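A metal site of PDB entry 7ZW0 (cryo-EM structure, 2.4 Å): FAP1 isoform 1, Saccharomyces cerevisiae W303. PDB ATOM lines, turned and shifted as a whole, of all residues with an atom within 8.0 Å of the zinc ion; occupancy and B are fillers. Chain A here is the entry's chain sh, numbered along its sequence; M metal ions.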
ATOM      1  N   MET A  69      -1.992  -8.141 -11.741  1.00  0.00           N
ATOM      2  CA  MET A  69      -1.266  -7.324 -10.769  1.00  0.00           C
ATOM      3  C   MET A  69      -1.344  -7.749  -9.309  1.00  0.00           C
ATOM      4  O   MET A  69      -0.330  -7.736  -8.614  1.00  0.00           O
ATOM      5  CB  MET A  69      -1.682  -5.859 -10.908  1.00  0.00           C
ATOM      6  CG  MET A  69      -1.324  -5.258 -12.253  1.00  0.00           C
ATOM      7  SD  MET A  69      -1.648  -3.485 -12.369  1.00  0.00           S
ATOM      8  CE  MET A  69      -0.529  -2.856 -11.121  1.00  0.00           C
ATOM      9  N   PHE A  82     -10.182  -8.678 -15.723  1.00  0.00           N
ATOM     10  CA  PHE A  82     -10.992  -7.500 -15.375  1.00  0.00           C
ATOM     11  C   PHE A  82     -10.390  -6.232 -15.987  1.00  0.00           C
ATOM     12  O   PHE A  82      -9.175  -6.037 -15.915  1.00  0.00           O
ATOM     13  CB  PHE A  82     -11.084  -7.334 -13.874  1.00  0.00           C
ATOM     14  CG  PHE A  82     -11.839  -6.103 -13.451  1.00  0.00           C
ATOM     15  CD1 PHE A  82     -13.218  -6.079 -13.510  1.00  0.00           C
ATOM     16  CD2 PHE A  82     -11.172  -4.989 -12.988  1.00  0.00           C
ATOM     17  CE1 PHE A  82     -13.927  -4.950 -13.126  1.00  0.00           C
ATOM     18  CE2 PHE A  82     -11.860  -3.855 -12.612  1.00  0.00           C
ATOM     19  CZ  PHE A  82     -13.237  -3.841 -12.671  1.00  0.00           C
ATOM     20  N   ALA A  83     -11.214  -5.391 -16.590  1.00  0.00           N
ATOM     21  CA  ALA A  83     -10.706  -4.195 -17.249  1.00  0.00           C
ATOM     22  C   ALA A  83     -11.220  -2.920 -16.617  1.00  0.00           C
ATOM     23  O   ALA A  83     -12.401  -2.812 -16.289  1.00  0.00           O
ATOM     24  CB  ALA A  83     -11.026  -4.230 -18.727  1.00  0.00           C
ATOM     25  N   CYS A  84     -10.345  -1.942 -16.453  1.00  0.00           N
ATOM     26  CA  CYS A  84     -10.762  -0.655 -15.914  1.00  0.00           C
ATOM     27  C   CYS A  84     -10.527   0.389 -16.978  1.00  0.00           C
ATOM     28  O   CYS A  84      -9.459   0.420 -17.572  1.00  0.00           O
ATOM     29  CB  CYS A  84      -9.984  -0.299 -14.647  1.00  0.00           C
ATOM     30  SG  CYS A  84     -10.268   1.377 -14.050  1.00  0.00           S
ATOM     31  N   LYS A  85     -11.504   1.244 -17.231  1.00  0.00           N
ATOM     32  CA  LYS A  85     -11.365   2.214 -18.303  1.00  0.00           C
ATOM     33  C   LYS A  85     -10.227   3.181 -18.050  1.00  0.00           C
ATOM     34  O   LYS A  85      -9.497   3.537 -18.962  1.00  0.00           O
ATOM     35  CB  LYS A  85     -12.679   2.993 -18.501  1.00  0.00           C
ATOM     36  CG  LYS A  85     -13.764   2.236 -19.268  1.00  0.00           C
ATOM     37  CD  LYS A  85     -14.537   1.265 -18.382  1.00  0.00           C
ATOM     38  CE  LYS A  85     -14.195  -0.173 -18.699  1.00  0.00           C
ATOM     39  NZ  LYS A  85     -14.682  -1.100 -17.641  1.00  0.00           N
ATOM     40  N   ARG A  86     -10.059   3.603 -16.805  1.00  0.00           N
ATOM     41  CA  ARG A  86      -9.031   4.585 -16.499  1.00  0.00           C
ATOM     42  C   ARG A  86      -7.615   4.068 -16.789  1.00  0.00           C
ATOM     43  O   ARG A  86      -6.799   4.791 -17.367  1.00  0.00           O
ATOM     44  CB  ARG A  86      -9.156   5.051 -15.044  1.00  0.00           C
ATOM     45  CG  ARG A  86      -8.427   6.355 -14.753  1.00  0.00           C
ATOM     46  CD  ARG A  86      -9.006   7.499 -15.563  1.00  0.00           C
ATOM     47  NE  ARG A  86      -8.098   8.640 -15.633  1.00  0.00           N
ATOM     48  CZ  ARG A  86      -7.214   8.836 -16.608  1.00  0.00           C
ATOM     49  NH1 ARG A  86      -7.125   7.969 -17.603  1.00  0.00           N
ATOM     50  NH2 ARG A  86      -6.419   9.900 -16.588  1.00  0.00           N
ATOM     51  N   CYS A  87      -7.331   2.829 -16.414  1.00  0.00           N
ATOM     52  CA  CYS A  87      -6.002   2.271 -16.661  1.00  0.00           C
ATOM     53  C   CYS A  87      -5.910   1.375 -17.877  1.00  0.00           C
ATOM     54  O   CYS A  87      -4.802   1.035 -18.296  1.00  0.00           O
ATOM     55  CB  CYS A  87      -5.542   1.468 -15.452  1.00  0.00           C
ATOM     56  SG  CYS A  87      -6.440  -0.082 -15.229  1.00  0.00           S
ATOM     57  N   TYR A  88      -7.038   1.018 -18.468  1.00  0.00           N
ATOM     58  CA  TYR A  88      -7.044   0.068 -19.581  1.00  0.00           C
ATOM     59  C   TYR A  88      -6.031  -1.055 -19.402  1.00  0.00           C
ATOM     60  O   TYR A  88      -5.278  -1.381 -20.327  1.00  0.00           O
ATOM     61  CB  TYR A  88      -6.896   0.776 -20.930  1.00  0.00           C
ATOM     62  CG  TYR A  88      -8.208   1.330 -21.423  1.00  0.00           C
ATOM     63  CD1 TYR A  88      -9.336   0.519 -21.472  1.00  0.00           C
ATOM     64  CD2 TYR A  88      -8.320   2.640 -21.845  1.00  0.00           C
ATOM     65  CE1 TYR A  88     -10.546   1.014 -21.920  1.00  0.00           C
ATOM     66  CE2 TYR A  88      -9.522   3.147 -22.292  1.00  0.00           C
ATOM     67  CZ  TYR A  88     -10.639   2.328 -22.320  1.00  0.00           C
ATOM     68  OH  TYR A  88     -11.839   2.826 -22.767  1.00  0.00           O
ATOM     69  N   ARG A  89      -6.014  -1.662 -18.220  1.00  0.00           N
ATOM     70  CA  ARG A  89      -5.099  -2.748 -17.937  1.00  0.00           C
ATOM     71  C   ARG A  89      -5.921  -3.922 -17.420  1.00  0.00           C
ATOM     72  O   ARG A  89      -7.024  -3.725 -16.903  1.00  0.00           O
ATOM     73  CB  ARG A  89      -4.061  -2.280 -16.909  1.00  0.00           C
ATOM     74  CG  ARG A  89      -3.355  -3.353 -16.099  1.00  0.00           C
ATOM     75  CD  ARG A  89      -1.943  -3.603 -16.594  1.00  0.00           C
ATOM     76  NE  ARG A  89      -1.319  -4.726 -15.901  1.00  0.00           N
ATOM     77  CZ  ARG A  89      -0.055  -5.113 -16.079  1.00  0.00           C
ATOM     78  NH1 ARG A  89       0.723  -4.449 -16.922  1.00  0.00           N
ATOM     79  NH2 ARG A  89       0.420  -6.157 -15.416  1.00  0.00           N
ATOM     80  N   VAL A  90      -5.417  -5.140 -17.550  1.00  0.00           N
ATOM     81  CA  VAL A  90      -6.169  -6.319 -17.128  1.00  0.00           C
ATOM     82  C   VAL A  90      -5.534  -7.134 -16.006  1.00  0.00           C
ATOM     83  O   VAL A  90      -4.314  -7.348 -15.993  1.00  0.00           O
ATOM     84  CB  VAL A  90      -6.512  -7.202 -18.335  1.00  0.00           C
ATOM     85  CG1 VAL A  90      -6.641  -8.659 -17.964  1.00  0.00           C
ATOM     86  CG2 VAL A  90      -7.780  -6.698 -18.987  1.00  0.00           C
ATOM     87  N   PHE A  91      -6.338  -7.548 -15.030  1.00  0.00           N
ATOM     88  CA  PHE A  91      -5.836  -8.362 -13.929  1.00  0.00           C
ATOM     89  C   PHE A  91      -6.750  -9.565 -13.860  1.00  0.00           C
ATOM     90  O   PHE A  91      -7.786  -9.583 -14.507  1.00  0.00           O
ATOM     91  CB  PHE A  91      -5.919  -7.587 -12.614  1.00  0.00           C
ATOM     92  CG  PHE A  91      -6.118  -6.113 -12.788  1.00  0.00           C
ATOM     93  CD1 PHE A  91      -7.401  -5.585 -12.909  1.00  0.00           C
ATOM     94  CD2 PHE A  91      -5.036  -5.251 -12.831  1.00  0.00           C
ATOM     95  CE1 PHE A  91      -7.586  -4.221 -13.074  1.00  0.00           C
ATOM     96  CE2 PHE A  91      -5.219  -3.897 -12.986  1.00  0.00           C
ATOM     97  CZ  PHE A  91      -6.500  -3.378 -13.118  1.00  0.00           C
ATOM     98  N   ILE A  96      -8.465  -9.347  -8.533  1.00  0.00           N
ATOM     99  CA  ILE A  96      -8.798  -7.947  -8.357  1.00  0.00           C
ATOM    100  C   ILE A  96     -10.009  -7.777  -7.428  1.00  0.00           C
ATOM    101  O   ILE A  96     -10.107  -6.767  -6.732  1.00  0.00           O
ATOM    102  CB  ILE A  96      -9.011  -7.230  -9.711  1.00  0.00           C
ATOM    103  CG1 ILE A  96      -8.811  -5.718  -9.564  1.00  0.00           C
ATOM    104  CG2 ILE A  96     -10.396  -7.502 -10.288  1.00  0.00           C
ATOM    105  CD1 ILE A  96      -7.422  -5.332  -9.114  1.00  0.00           C
ATOM    106  N   TRP A 112     -13.662   0.674  -3.690  1.00  0.00           N
ATOM    107  CA  TRP A 112     -12.588  -0.155  -4.232  1.00  0.00           C
ATOM    108  C   TRP A 112     -11.598   0.660  -5.076  1.00  0.00           C
ATOM    109  O   TRP A 112     -11.987   1.631  -5.705  1.00  0.00           O
ATOM    110  CB  TRP A 112     -13.178  -1.311  -5.041  1.00  0.00           C
ATOM    111  CG  TRP A 112     -13.136  -1.130  -6.519  1.00  0.00           C
ATOM    112  CD1 TRP A 112     -14.024  -0.447  -7.290  1.00  0.00           C
ATOM    113  CD2 TRP A 112     -12.144  -1.658  -7.421  1.00  0.00           C
ATOM    114  NE1 TRP A 112     -13.649  -0.519  -8.608  1.00  0.00           N
ATOM    115  CE2 TRP A 112     -12.497  -1.250  -8.711  1.00  0.00           C
ATOM    116  CE3 TRP A 112     -10.994  -2.433  -7.244  1.00  0.00           C
ATOM    117  CZ2 TRP A 112     -11.748  -1.587  -9.828  1.00  0.00           C
ATOM    118  CZ3 TRP A 112     -10.257  -2.762  -8.351  1.00  0.00           C
ATOM    119  CH2 TRP A 112     -10.623  -2.347  -9.633  1.00  0.00           C
ATOM    120  N   LYS A 113     -10.323   0.264  -5.102  1.00  0.00           N
ATOM    121  CA  LYS A 113      -9.317   1.061  -5.835  1.00  0.00           C
ATOM    122  C   LYS A 113      -8.620   0.272  -6.935  1.00  0.00           C
ATOM    123  O   LYS A 113      -8.270  -0.880  -6.734  1.00  0.00           O
ATOM    124  CB  LYS A 113      -8.273   1.613  -4.855  1.00  0.00           C
ATOM    125  CG  LYS A 113      -7.341   2.649  -5.468  1.00  0.00           C
ATOM    126  CD  LYS A 113      -6.678   3.482  -4.389  1.00  0.00           C
ATOM    127  CE  LYS A 113      -6.063   4.733  -4.990  1.00  0.00           C
ATOM    128  NZ  LYS A 113      -5.553   5.655  -3.931  1.00  0.00           N
ATOM    129  N   CYS A 114      -8.415   0.888  -8.080  1.00  0.00           N
ATOM    130  CA  CYS A 114      -7.708   0.224  -9.157  1.00  0.00           C
ATOM    131  C   CYS A 114      -6.246   0.609  -9.113  1.00  0.00           C
ATOM    132  O   CYS A 114      -5.917   1.782  -9.245  1.00  0.00           O
ATOM    133  CB  CYS A 114      -8.306   0.597 -10.505  1.00  0.00           C
ATOM    134  SG  CYS A 114      -7.515  -0.241 -11.890  1.00  0.00           S
ATOM    135  N   PRO A 115      -5.347  -0.366  -8.949  1.00  0.00           N
ATOM    136  CA  PRO A 115      -3.915  -0.071  -8.789  1.00  0.00           C
ATOM    137  C   PRO A 115      -3.177   0.565  -9.966  1.00  0.00           C
ATOM    138  O   PRO A 115      -2.372   1.466  -9.728  1.00  0.00           O
ATOM    139  CB  PRO A 115      -3.292  -1.448  -8.523  1.00  0.00           C
ATOM    140  CG  PRO A 115      -4.436  -2.337  -8.133  1.00  0.00           C
ATOM    141  CD  PRO A 115      -5.619  -1.813  -8.879  1.00  0.00           C
ATOM    142  N   ASN A 116      -3.425   0.125 -11.186  1.00  0.00           N
ATOM    143  CA  ASN A 116      -2.645   0.647 -12.312  1.00  0.00           C
ATOM    144  C   ASN A 116      -2.843   2.131 -12.525  1.00  0.00           C
ATOM    145  O   ASN A 116      -1.881   2.865 -12.771  1.00  0.00           O
ATOM    146  CB  ASN A 116      -2.956  -0.126 -13.595  1.00  0.00           C
ATOM    147  CG  ASN A 116      -1.863   0.037 -14.645  1.00  0.00           C
ATOM    148  OD1 ASN A 116      -0.687  -0.209 -14.365  1.00  0.00           O
ATOM    149  ND2 ASN A 116      -2.250   0.426 -15.848  1.00  0.00           N
ATOM    150  N   CYS A 117      -4.078   2.597 -12.424  1.00  0.00           N
ATOM    151  CA  CYS A 117      -4.343   4.025 -12.543  1.00  0.00           C
ATOM    152  C   CYS A 117      -4.357   4.661 -11.176  1.00  0.00           C
ATOM    153  O   CYS A 117      -4.579   5.871 -11.066  1.00  0.00           O
ATOM    154  CB  CYS A 117      -5.671   4.269 -13.245  1.00  0.00           C
ATOM    155  SG  CYS A 117      -6.990   3.185 -12.682  1.00  0.00           S
ATOM    156  N   TYR A 118      -4.142   3.864 -10.135  1.00  0.00           N
ATOM    157  CA  TYR A 118      -4.198   4.367  -8.764  1.00  0.00           C
ATOM    158  C   TYR A 118      -5.471   5.174  -8.638  1.00  0.00           C
ATOM    159  O   TYR A 118      -5.466   6.280  -8.103  1.00  0.00           O
ATOM    160  CB  TYR A 118      -2.955   5.214  -8.436  1.00  0.00           C
ATOM    161  CG  TYR A 118      -2.645   5.298  -6.968  1.00  0.00           C
ATOM    162  CD1 TYR A 118      -2.381   4.154  -6.221  1.00  0.00           C
ATOM    163  CD2 TYR A 118      -2.605   6.524  -6.317  1.00  0.00           C
ATOM    164  CE1 TYR A 118      -2.101   4.232  -4.875  1.00  0.00           C
ATOM    165  CE2 TYR A 118      -2.318   6.614  -4.970  1.00  0.00           C
ATOM    166  CZ  TYR A 118      -2.058   5.459  -4.254  1.00  0.00           C
ATOM    167  OH  TYR A 118      -1.769   5.539  -2.908  1.00  0.00           O
ATOM    168  N   TYR A 119      -6.573   4.627  -9.141  1.00  0.00           N
ATOM    169  CA  TYR A 119      -7.832   5.366  -9.136  1.00  0.00           C
ATOM    170  C   TYR A 119      -8.901   4.615  -8.396  1.00  0.00           C
ATOM    171  O   TYR A 119      -9.147   3.442  -8.670  1.00  0.00           O
ATOM    172  CB  TYR A 119      -8.237   5.691 -10.582  1.00  0.00           C
ATOM    173  CG  TYR A 119      -9.698   5.503 -10.952  1.00  0.00           C
ATOM    174  CD1 TYR A 119     -10.166   4.290 -11.433  1.00  0.00           C
ATOM    175  CD2 TYR A 119     -10.593   6.560 -10.874  1.00  0.00           C
ATOM    176  CE1 TYR A 119     -11.488   4.114 -11.783  1.00  0.00           C
ATOM    177  CE2 TYR A 119     -11.916   6.393 -11.224  1.00  0.00           C
ATOM    178  CZ  TYR A 119     -12.355   5.177 -11.672  1.00  0.00           C
ATOM    179  OH  TYR A 119     -13.677   5.000 -12.022  1.00  0.00           O
ATOM    180  N   VAL A 120      -9.525   5.268  -7.425  1.00  0.00           N
ATOM    181  CA  VAL A 120     -10.608   4.628  -6.694  1.00  0.00           C
ATOM    182  C   VAL A 120     -11.888   4.647  -7.498  1.00  0.00           C
ATOM    183  O   VAL A 120     -12.164   5.603  -8.210  1.00  0.00           O
ATOM    184  CB  VAL A 120     -10.852   5.335  -5.353  1.00  0.00           C
ATOM    185  CG1 VAL A 120     -10.676   4.354  -4.198  1.00  0.00           C
ATOM    186  CG2 VAL A 120      -9.906   6.504  -5.200  1.00  0.00           C
ATOM    187  N   SER A 121     -12.688   3.602  -7.378  1.00  0.00           N
ATOM    188  CA  SER A 121     -13.983   3.556  -8.054  1.00  0.00           C
ATOM    189  C   SER A 121     -15.007   3.143  -7.023  1.00  0.00           C
ATOM    190  O   SER A 121     -14.632   2.669  -5.943  1.00  0.00           O
ATOM    191  CB  SER A 121     -13.955   2.625  -9.265  1.00  0.00           C
ATOM    192  OG  SER A 121     -15.185   2.666  -9.975  1.00  0.00           O
HETATM  193 ZN    ZN M   1      -7.840   0.893 -13.564  1.00  0.00          ZN
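SG of Cys 114 is bound to the zinc ion, at 2.0 Å. SG of Cys 87 is bound to the zinc ion (2.4 Å). The zinc ion is bound by SG of Cys 84 (2.5 Å). The zinc ion is bound by SG of Cys 117, at 2.6 Å. The zinc ion has four donor atoms within binding distance.
N of Cys 114 is in hydrogen-bond range of O of Tyr 119, at 2.7 Å. SG of Cys 87 sits close to N of Arg 89, 3.4 Å away. SG of Cys 84 sits close to N of Arg 86 (3.5 Å).
Of the 22 residues printed, 4 come within 4 Å of the zinc ion. The nearest printed residue that does not touch the zinc ion is Phe 91 (4.5 Å).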
